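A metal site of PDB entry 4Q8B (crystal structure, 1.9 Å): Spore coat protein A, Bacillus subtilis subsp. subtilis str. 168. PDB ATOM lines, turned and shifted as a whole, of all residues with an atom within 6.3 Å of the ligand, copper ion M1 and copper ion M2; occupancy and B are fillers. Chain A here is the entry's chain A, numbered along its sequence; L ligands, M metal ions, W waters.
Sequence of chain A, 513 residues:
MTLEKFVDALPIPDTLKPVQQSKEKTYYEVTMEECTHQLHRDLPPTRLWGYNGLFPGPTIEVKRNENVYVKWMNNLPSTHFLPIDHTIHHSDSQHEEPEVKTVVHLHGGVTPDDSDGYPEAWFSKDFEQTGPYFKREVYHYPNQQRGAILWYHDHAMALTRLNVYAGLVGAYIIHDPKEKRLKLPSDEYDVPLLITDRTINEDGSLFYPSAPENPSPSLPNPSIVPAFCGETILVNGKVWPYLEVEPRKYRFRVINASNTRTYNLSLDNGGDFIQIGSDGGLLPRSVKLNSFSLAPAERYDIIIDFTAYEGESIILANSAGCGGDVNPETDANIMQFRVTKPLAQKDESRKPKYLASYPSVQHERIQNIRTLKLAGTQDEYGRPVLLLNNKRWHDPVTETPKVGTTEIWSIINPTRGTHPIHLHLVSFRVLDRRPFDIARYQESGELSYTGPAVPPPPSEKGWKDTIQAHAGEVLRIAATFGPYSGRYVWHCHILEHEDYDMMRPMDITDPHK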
ATOM      1  N   HIS A 105       0.536  -9.961 -21.944  1.00  0.00           N
ATOM      2  CA  HIS A 105       0.637  -9.069 -23.075  1.00  0.00           C
ATOM      3  C   HIS A 105       0.517  -7.658 -22.582  1.00  0.00           C
ATOM      4  O   HIS A 105      -0.448  -7.325 -21.903  1.00  0.00           O
ATOM      5  CB  HIS A 105      -0.480  -9.366 -24.064  1.00  0.00           C
ATOM      6  CG  HIS A 105      -0.583  -8.401 -25.211  1.00  0.00           C
ATOM      7  ND1 HIS A 105       0.459  -8.145 -26.081  1.00  0.00           N
ATOM      8  CD2 HIS A 105      -1.609  -7.616 -25.610  1.00  0.00           C
ATOM      9  CE1 HIS A 105       0.076  -7.251 -26.977  1.00  0.00           C
ATOM     10  NE2 HIS A 105      -1.185  -6.925 -26.705  1.00  0.00           N
ATOM     11  N   LEU A 106       1.467  -6.835 -22.986  1.00  0.00           N
ATOM     12  CA  LEU A 106       1.408  -5.405 -22.864  1.00  0.00           C
ATOM     13  C   LEU A 106       0.649  -4.819 -24.065  1.00  0.00           C
ATOM     14  O   LEU A 106       1.213  -4.694 -25.165  1.00  0.00           O
ATOM     15  CB  LEU A 106       2.825  -4.791 -22.742  1.00  0.00           C
ATOM     16  CG  LEU A 106       2.891  -3.272 -22.612  1.00  0.00           C
ATOM     17  CD1 LEU A 106       2.094  -2.782 -21.402  1.00  0.00           C
ATOM     18  CD2 LEU A 106       4.319  -2.771 -22.482  1.00  0.00           C
ATOM     19  N   HIS A 107      -0.612  -4.478 -23.841  1.00  0.00           N
ATOM     20  CA  HIS A 107      -1.507  -4.046 -24.883  1.00  0.00           C
ATOM     21  C   HIS A 107      -1.128  -2.663 -25.275  1.00  0.00           C
ATOM     22  O   HIS A 107      -1.126  -1.748 -24.455  1.00  0.00           O
ATOM     23  CB  HIS A 107      -2.972  -4.098 -24.437  1.00  0.00           C
ATOM     24  CG  HIS A 107      -3.943  -3.740 -25.484  1.00  0.00           C
ATOM     25  ND1 HIS A 107      -4.948  -4.587 -25.899  1.00  0.00           N
ATOM     26  CD2 HIS A 107      -4.037  -2.641 -26.274  1.00  0.00           C
ATOM     27  CE1 HIS A 107      -5.634  -4.021 -26.868  1.00  0.00           C
ATOM     28  NE2 HIS A 107      -5.085  -2.851 -27.119  1.00  0.00           N
ATOM     29  N   GLY A 108      -0.814  -2.533 -26.543  1.00  0.00           N
ATOM     30  CA  GLY A 108      -0.218  -1.300 -27.087  1.00  0.00           C
ATOM     31  C   GLY A 108       1.303  -1.223 -27.100  1.00  0.00           C
ATOM     32  O   GLY A 108       1.854  -0.285 -27.612  1.00  0.00           O
ATOM     33  N   GLY A 109       1.998  -2.194 -26.519  1.00  0.00           N
ATOM     34  CA  GLY A 109       3.458  -2.113 -26.437  1.00  0.00           C
ATOM     35  C   GLY A 109       4.055  -2.222 -27.840  1.00  0.00           C
ATOM     36  O   GLY A 109       3.666  -3.047 -28.635  1.00  0.00           O
ATOM     37  N   ASP A 116       6.095 -10.073 -26.480  1.00  0.00           N
ATOM     38  CA  ASP A 116       4.756  -9.533 -26.714  1.00  0.00           C
ATOM     39  C   ASP A 116       3.650 -10.314 -26.055  1.00  0.00           C
ATOM     40  O   ASP A 116       2.521  -9.863 -26.024  1.00  0.00           O
ATOM     41  CB  ASP A 116       4.476  -9.479 -28.206  1.00  0.00           C
ATOM     42  CG  ASP A 116       3.249  -8.614 -28.563  1.00  0.00           C
ATOM     43  OD1 ASP A 116       3.128  -7.471 -28.032  1.00  0.00           O
ATOM     44  OD2 ASP A 116       2.456  -9.094 -29.391  1.00  0.00           O
ATOM     45  N   TRP A 151      -2.037  -1.017 -21.275  1.00  0.00           N
ATOM     46  CA  TRP A 151      -2.460  -1.820 -20.164  1.00  0.00           C
ATOM     47  C   TRP A 151      -1.967  -3.224 -20.405  1.00  0.00           C
ATOM     48  O   TRP A 151      -1.596  -3.580 -21.531  1.00  0.00           O
ATOM     49  CB  TRP A 151      -3.993  -1.775 -19.979  1.00  0.00           C
ATOM     50  CG  TRP A 151      -4.884  -2.300 -21.050  1.00  0.00           C
ATOM     51  CD1 TRP A 151      -4.944  -1.884 -22.339  1.00  0.00           C
ATOM     52  CD2 TRP A 151      -5.845  -3.356 -20.934  1.00  0.00           C
ATOM     53  NE1 TRP A 151      -5.876  -2.581 -23.014  1.00  0.00           N
ATOM     54  CE2 TRP A 151      -6.455  -3.499 -22.174  1.00  0.00           C
ATOM     55  CE3 TRP A 151      -6.249  -4.210 -19.895  1.00  0.00           C
ATOM     56  CZ2 TRP A 151      -7.448  -4.433 -22.414  1.00  0.00           C
ATOM     57  CZ3 TRP A 151      -7.216  -5.131 -20.137  1.00  0.00           C
ATOM     58  CH2 TRP A 151      -7.813  -5.234 -21.389  1.00  0.00           C
ATOM     59  N   HIS A 153      -2.420  -7.523 -19.506  1.00  0.00           N
ATOM     60  CA  HIS A 153      -3.432  -8.486 -19.195  1.00  0.00           C
ATOM     61  C   HIS A 153      -3.024  -9.848 -19.685  1.00  0.00           C
ATOM     62  O   HIS A 153      -2.156  -9.998 -20.604  1.00  0.00           O
ATOM     63  CB  HIS A 153      -4.789  -8.084 -19.798  1.00  0.00           C
ATOM     64  CG  HIS A 153      -4.849  -7.981 -21.293  1.00  0.00           C
ATOM     65  ND1 HIS A 153      -4.975  -9.074 -22.108  1.00  0.00           N
ATOM     66  CD2 HIS A 153      -4.880  -6.902 -22.115  1.00  0.00           C
ATOM     67  CE1 HIS A 153      -5.014  -8.699 -23.376  1.00  0.00           C
ATOM     68  NE2 HIS A 153      -5.032  -7.377 -23.392  1.00  0.00           N
ATOM     69  N   ASP A 154      -3.669 -10.861 -19.133  1.00  0.00           N
ATOM     70  CA  ASP A 154      -3.407 -12.236 -19.578  1.00  0.00           C
ATOM     71  C   ASP A 154      -3.838 -12.464 -21.036  1.00  0.00           C
ATOM     72  O   ASP A 154      -4.739 -11.815 -21.545  1.00  0.00           O
ATOM     73  CB  ASP A 154      -4.069 -13.278 -18.711  1.00  0.00           C
ATOM     74  CG  ASP A 154      -3.557 -14.666 -19.032  1.00  0.00           C
ATOM     75  OD1 ASP A 154      -4.217 -15.367 -19.821  1.00  0.00           O
ATOM     76  OD2 ASP A 154      -2.443 -14.975 -18.544  1.00  0.00           O
ATOM     77  N   HIS A 155      -3.100 -13.321 -21.732  1.00  0.00           N
ATOM     78  CA  HIS A 155      -3.375 -13.563 -23.141  1.00  0.00           C
ATOM     79  C   HIS A 155      -3.218 -15.027 -23.488  1.00  0.00           C
ATOM     80  O   HIS A 155      -3.001 -15.367 -24.628  1.00  0.00           O
ATOM     81  CB  HIS A 155      -2.408 -12.712 -23.997  1.00  0.00           C
ATOM     82  CG  HIS A 155      -2.964 -12.246 -25.323  1.00  0.00           C
ATOM     83  ND1 HIS A 155      -3.424 -13.114 -26.293  1.00  0.00           N
ATOM     84  CD2 HIS A 155      -3.085 -11.004 -25.858  1.00  0.00           C
ATOM     85  CE1 HIS A 155      -3.802 -12.419 -27.361  1.00  0.00           C
ATOM     86  NE2 HIS A 155      -3.598 -11.145 -27.125  1.00  0.00           N
ATOM     87  N   THR A 160      -8.083 -16.681 -22.326  1.00  0.00           N
ATOM     88  CA  THR A 160      -7.995 -15.257 -22.088  1.00  0.00           C
ATOM     89  C   THR A 160      -9.240 -14.668 -21.410  1.00  0.00           C
ATOM     90  O   THR A 160      -9.140 -13.840 -20.454  1.00  0.00           O
ATOM     91  CB  THR A 160      -7.640 -14.558 -23.431  1.00  0.00           C
ATOM     92  OG1 THR A 160      -6.320 -15.002 -23.816  1.00  0.00           O
ATOM     93  CG2 THR A 160      -7.626 -13.035 -23.229  1.00  0.00           C
ATOM     94  N   ALA A 297     -10.907  -2.891 -24.550  1.00  0.00           N
ATOM     95  CA  ALA A 297      -9.506  -2.517 -24.824  1.00  0.00           C
ATOM     96  C   ALA A 297      -9.247  -1.114 -25.349  1.00  0.00           C
ATOM     97  O   ALA A 297      -8.082  -0.738 -25.499  1.00  0.00           O
ATOM     98  CB  ALA A 297      -8.784  -3.533 -25.700  1.00  0.00           C
ATOM     99  N   HIS A 422      -8.240  -5.364 -32.841  1.00  0.00           N
ATOM    100  CA  HIS A 422      -6.931  -4.988 -32.306  1.00  0.00           C
ATOM    101  C   HIS A 422      -5.813  -5.657 -33.097  1.00  0.00           C
ATOM    102  O   HIS A 422      -5.842  -6.860 -33.363  1.00  0.00           O
ATOM    103  CB  HIS A 422      -6.846  -5.376 -30.831  1.00  0.00           C
ATOM    104  CG  HIS A 422      -5.522  -5.128 -30.190  1.00  0.00           C
ATOM    105  ND1 HIS A 422      -4.844  -3.938 -30.248  1.00  0.00           N
ATOM    106  CD2 HIS A 422      -4.743  -5.969 -29.442  1.00  0.00           C
ATOM    107  CE1 HIS A 422      -3.717  -4.035 -29.567  1.00  0.00           C
ATOM    108  NE2 HIS A 422      -3.643  -5.255 -29.060  1.00  0.00           N
ATOM    109  N   LEU A 423      -4.825  -4.861 -33.474  1.00  0.00           N
ATOM    110  CA  LEU A 423      -3.608  -5.353 -34.051  1.00  0.00           C
ATOM    111  C   LEU A 423      -2.519  -5.154 -33.026  1.00  0.00           C
ATOM    112  O   LEU A 423      -2.370  -4.056 -32.457  1.00  0.00           O
ATOM    113  CB  LEU A 423      -3.233  -4.565 -35.301  1.00  0.00           C
ATOM    114  CG  LEU A 423      -3.894  -4.892 -36.625  1.00  0.00           C
ATOM    115  CD1 LEU A 423      -5.417  -4.824 -36.590  1.00  0.00           C
ATOM    116  CD2 LEU A 423      -3.328  -3.990 -37.731  1.00  0.00           C
ATOM    117  N   HIS A 424      -1.749  -6.199 -32.786  1.00  0.00           N
ATOM    118  CA  HIS A 424      -0.564  -6.000 -31.960  1.00  0.00           C
ATOM    119  C   HIS A 424       0.492  -5.190 -32.652  1.00  0.00           C
ATOM    120  O   HIS A 424       0.379  -4.929 -33.871  1.00  0.00           O
ATOM    121  CB  HIS A 424       0.056  -7.326 -31.550  1.00  0.00           C
ATOM    122  CG  HIS A 424      -0.769  -8.083 -30.574  1.00  0.00           C
ATOM    123  ND1 HIS A 424      -0.213  -8.885 -29.599  1.00  0.00           N
ATOM    124  CD2 HIS A 424      -2.111  -8.136 -30.396  1.00  0.00           C
ATOM    125  CE1 HIS A 424      -1.189  -9.468 -28.908  1.00  0.00           C
ATOM    126  NE2 HIS A 424      -2.343  -8.998 -29.344  1.00  0.00           N
ATOM    127  N   LEU A 425       1.500  -4.817 -31.856  1.00  0.00           N
ATOM    128  CA  LEU A 425       2.692  -4.004 -32.229  1.00  0.00           C
ATOM    129  C   LEU A 425       2.449  -2.542 -32.674  1.00  0.00           C
ATOM    130  O   LEU A 425       3.083  -1.629 -32.188  1.00  0.00           O
ATOM    131  CB  LEU A 425       3.530  -4.695 -33.301  1.00  0.00           C
ATOM    132  CG  LEU A 425       4.775  -3.929 -33.714  1.00  0.00           C
ATOM    133  CD1 LEU A 425       5.791  -3.935 -32.615  1.00  0.00           C
ATOM    134  CD2 LEU A 425       5.333  -4.469 -35.013  1.00  0.00           C
ATOM    135  N   ASP A 465      -5.228   1.537 -31.694  1.00  0.00           N
ATOM    136  CA  ASP A 465      -4.780   0.155 -31.812  1.00  0.00           C
ATOM    137  C   ASP A 465      -5.944  -0.806 -31.703  1.00  0.00           C
ATOM    138  O   ASP A 465      -5.822  -1.988 -32.044  1.00  0.00           O
ATOM    139  CB  ASP A 465      -3.586  -0.160 -30.913  1.00  0.00           C
ATOM    140  CG  ASP A 465      -3.894  -0.150 -29.430  1.00  0.00           C
ATOM    141  OD1 ASP A 465      -4.961  -0.640 -29.025  1.00  0.00           O
ATOM    142  OD2 ASP A 465      -3.023   0.382 -28.693  1.00  0.00           O
ATOM    143  N   VAL A 489       0.006 -11.089 -33.487  1.00  0.00           N
ATOM    144  CA  VAL A 489      -1.368 -11.513 -33.731  1.00  0.00           C
ATOM    145  C   VAL A 489      -2.233 -10.298 -33.977  1.00  0.00           C
ATOM    146  O   VAL A 489      -1.868  -9.120 -33.708  1.00  0.00           O
ATOM    147  CB  VAL A 489      -2.030 -12.340 -32.540  1.00  0.00           C
ATOM    148  CG1 VAL A 489      -1.169 -13.545 -32.128  1.00  0.00           C
ATOM    149  CG2 VAL A 489      -2.154 -11.477 -31.380  1.00  0.00           C
ATOM    150  N   TRP A 490      -3.424 -10.588 -34.468  1.00  0.00           N
ATOM    151  CA  TRP A 490      -4.493  -9.587 -34.530  1.00  0.00           C
ATOM    152  C   TRP A 490      -5.784 -10.331 -34.281  1.00  0.00           C
ATOM    153  O   TRP A 490      -5.896 -11.571 -34.554  1.00  0.00           O
ATOM    154  CB  TRP A 490      -4.482  -8.828 -35.915  1.00  0.00           C
ATOM    155  CG  TRP A 490      -5.047  -9.612 -37.120  1.00  0.00           C
ATOM    156  CD1 TRP A 490      -4.406 -10.615 -37.826  1.00  0.00           C
ATOM    157  CD2 TRP A 490      -6.286  -9.396 -37.788  1.00  0.00           C
ATOM    158  NE1 TRP A 490      -5.226 -11.073 -38.863  1.00  0.00           N
ATOM    159  CE2 TRP A 490      -6.371 -10.341 -38.858  1.00  0.00           C
ATOM    160  CE3 TRP A 490      -7.371  -8.521 -37.567  1.00  0.00           C
ATOM    161  CZ2 TRP A 490      -7.474 -10.392 -39.715  1.00  0.00           C
ATOM    162  CZ3 TRP A 490      -8.469  -8.604 -38.414  1.00  0.00           C
ATOM    163  CH2 TRP A 490      -8.517  -9.533 -39.473  1.00  0.00           C
ATOM    164  N   HIS A 491      -6.774  -9.642 -33.719  1.00  0.00           N
ATOM    165  CA  HIS A 491      -7.957 -10.294 -33.245  1.00  0.00           C
ATOM    166  C   HIS A 491      -9.036  -9.284 -32.818  1.00  0.00           C
ATOM    167  O   HIS A 491      -8.759  -8.077 -32.641  1.00  0.00           O
ATOM    168  CB  HIS A 491      -7.661 -11.210 -32.032  1.00  0.00           C
ATOM    169  CG  HIS A 491      -6.964 -10.527 -30.898  1.00  0.00           C
ATOM    170  ND1 HIS A 491      -7.634  -9.996 -29.807  1.00  0.00           N
ATOM    171  CD2 HIS A 491      -5.651 -10.302 -30.667  1.00  0.00           C
ATOM    172  CE1 HIS A 491      -6.765  -9.466 -28.970  1.00  0.00           C
ATOM    173  NE2 HIS A 491      -5.562  -9.640 -29.462  1.00  0.00           N
ATOM    174  N   HIS A 493     -11.259  -8.014 -29.839  1.00  0.00           N
ATOM    175  CA  HIS A 493     -10.972  -7.907 -28.396  1.00  0.00           C
ATOM    176  C   HIS A 493     -12.172  -8.108 -27.492  1.00  0.00           C
ATOM    177  O   HIS A 493     -12.046  -7.912 -26.276  1.00  0.00           O
ATOM    178  CB  HIS A 493     -10.257  -6.613 -28.067  1.00  0.00           C
ATOM    179  CG  HIS A 493      -9.249  -6.741 -26.972  1.00  0.00           C
ATOM    180  ND1 HIS A 493      -9.616  -7.034 -25.679  1.00  0.00           N
ATOM    181  CD2 HIS A 493      -7.909  -6.632 -26.965  1.00  0.00           C
ATOM    182  CE1 HIS A 493      -8.543  -7.098 -24.923  1.00  0.00           C
ATOM    183  NE2 HIS A 493      -7.495  -6.835 -25.672  1.00  0.00           N
ATOM    184  N   LEU A 495     -13.498 -10.855 -25.619  1.00  0.00           N
ATOM    185  CA  LEU A 495     -12.660 -12.006 -25.313  1.00  0.00           C
ATOM    186  C   LEU A 495     -13.343 -13.313 -25.611  1.00  0.00           C
ATOM    187  O   LEU A 495     -12.673 -14.339 -25.958  1.00  0.00           O
ATOM    188  CB  LEU A 495     -12.158 -11.972 -23.862  1.00  0.00           C
ATOM    189  CG  LEU A 495     -11.387 -10.701 -23.529  1.00  0.00           C
ATOM    190  CD1 LEU A 495     -10.914 -10.746 -22.069  1.00  0.00           C
ATOM    191  CD2 LEU A 495     -10.214 -10.490 -24.421  1.00  0.00           C
ATOM    192  N   GLU A 498     -12.493 -13.669 -29.367  1.00  0.00           N
ATOM    193  CA  GLU A 498     -11.059 -13.968 -29.401  1.00  0.00           C
ATOM    194  C   GLU A 498     -10.778 -15.450 -29.156  1.00  0.00           C
ATOM    195  O   GLU A 498     -10.003 -16.050 -29.909  1.00  0.00           O
ATOM    196  CB  GLU A 498     -10.328 -13.118 -28.361  1.00  0.00           C
ATOM    197  CG  GLU A 498      -8.809 -13.230 -28.429  1.00  0.00           C
ATOM    198  CD  GLU A 498      -8.109 -12.343 -27.410  1.00  0.00           C
ATOM    199  OE1 GLU A 498      -8.633 -11.249 -27.061  1.00  0.00           O
ATOM    200  OE2 GLU A 498      -6.997 -12.752 -26.990  1.00  0.00           O
ATOM    201  N   MET A 503      -9.120 -14.826 -33.848  1.00  0.00           N
ATOM    202  CA  MET A 503      -7.724 -14.389 -33.670  1.00  0.00           C
ATOM    203  C   MET A 503      -6.846 -15.085 -34.691  1.00  0.00           C
ATOM    204  O   MET A 503      -7.017 -16.266 -34.921  1.00  0.00           O
ATOM    205  CB  MET A 503      -7.265 -14.725 -32.210  1.00  0.00           C
ATOM    206  CG  MET A 503      -5.844 -14.347 -31.934  1.00  0.00           C
ATOM    207  SD  MET A 503      -5.394 -14.524 -30.176  1.00  0.00           S
ATOM    208  CE  MET A 503      -5.406 -16.297 -30.052  1.00  0.00           C
HETATM  209  O1  LIG L   1      -4.927  -8.474 -26.461  1.00  0.00           O
HETATM  210  O2  LIG L   1      -4.477  -7.527 -27.081  1.00  0.00           O
HETATM  211 CU    CU M   1      -3.993  -9.536 -28.309  1.00  0.00          CU
HETATM  212 CU    CU M   2      -2.512  -6.144 -27.839  1.00  0.00          CU
HETATM  213 CU    CU M   3      -5.483  -6.343 -24.988  1.00  0.00          CU
HETATM  214  O   HOH W   1      -0.370  -4.213 -28.772  1.00  0.00           O
HETATM  215  O   HOH W   2      -6.715 -10.064 -25.862  1.00  0.00           O
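N of His 422 sits at hydrogen-bond distance from O of His 491 (2.8 Å).
ND1 of His 422 lies close to NE2 of His 107, at 3.3 Å.
A ring nitrogen (ND1) of His 422 sits at hydrogen-bond distance from the backbone carbonyl oxygen of Asp 465, at 2.8 Å.
O of His 153 sits at hydrogen-bond distance from N of His 105.
ND1 of His 491 sits at hydrogen-bond distance from OE1 of Glu 498.
ND1 of His 424 is in hydrogen-bond range of OD2 of Asp 116 (2.7 Å).
A ring nitrogen (NE2) of His 107 lies within hydrogen-bond range of the side-chain carboxylate of Asp 465 (2.9 Å).
O of Trp 151 is in hydrogen-bond range of N of His 107, at 2.7 Å.
Residues that only touch copper ion M2: His 107 (3.5 Å).
Of the 24 residues printed, 4 come within 4 Å of copper ion M2.
ND1 of His 107 lies close to O2 of the ligand (3.2 Å).
A ring nitrogen (NE2) of His 153 sits close to an oxygen (O1) of the ligand.
A ring nitrogen (NE2) of His 493 sits close to an oxygen (O1) of the ligand (3.1 Å).
Hydrophobic or aromatic side chains that line the ligand: His 105, His 107, His 153, His 155, His 422, His 491 and His 493.
Eight residues have an atom within 4 Å of the ligand: His 105, His 107, His 153, His 155, His 422, His 424, His 491 and His 493.
Copper ion M2 is bound by NE2 of His 422 (1.9 Å), NE2 of His 105 (1.9 Å) and O2 of the ligand (2.5 Å).
Copper ion M2 has three donor atoms within binding distance.
Of the 24 residues printed, 4 come within 4 Å of copper ion M1.
The nearest printed residue that does not touch copper ion M1 is Val 489 (4.1 Å).
Copper ion M1 is bound by a ring nitrogen (NE2) of His 491, a ring nitrogen (NE2) of His 424, a ring nitrogen (NE2) of His 155 and an oxygen (O1) of the ligand.
Copper ion M1 has four donor atoms within binding distance.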
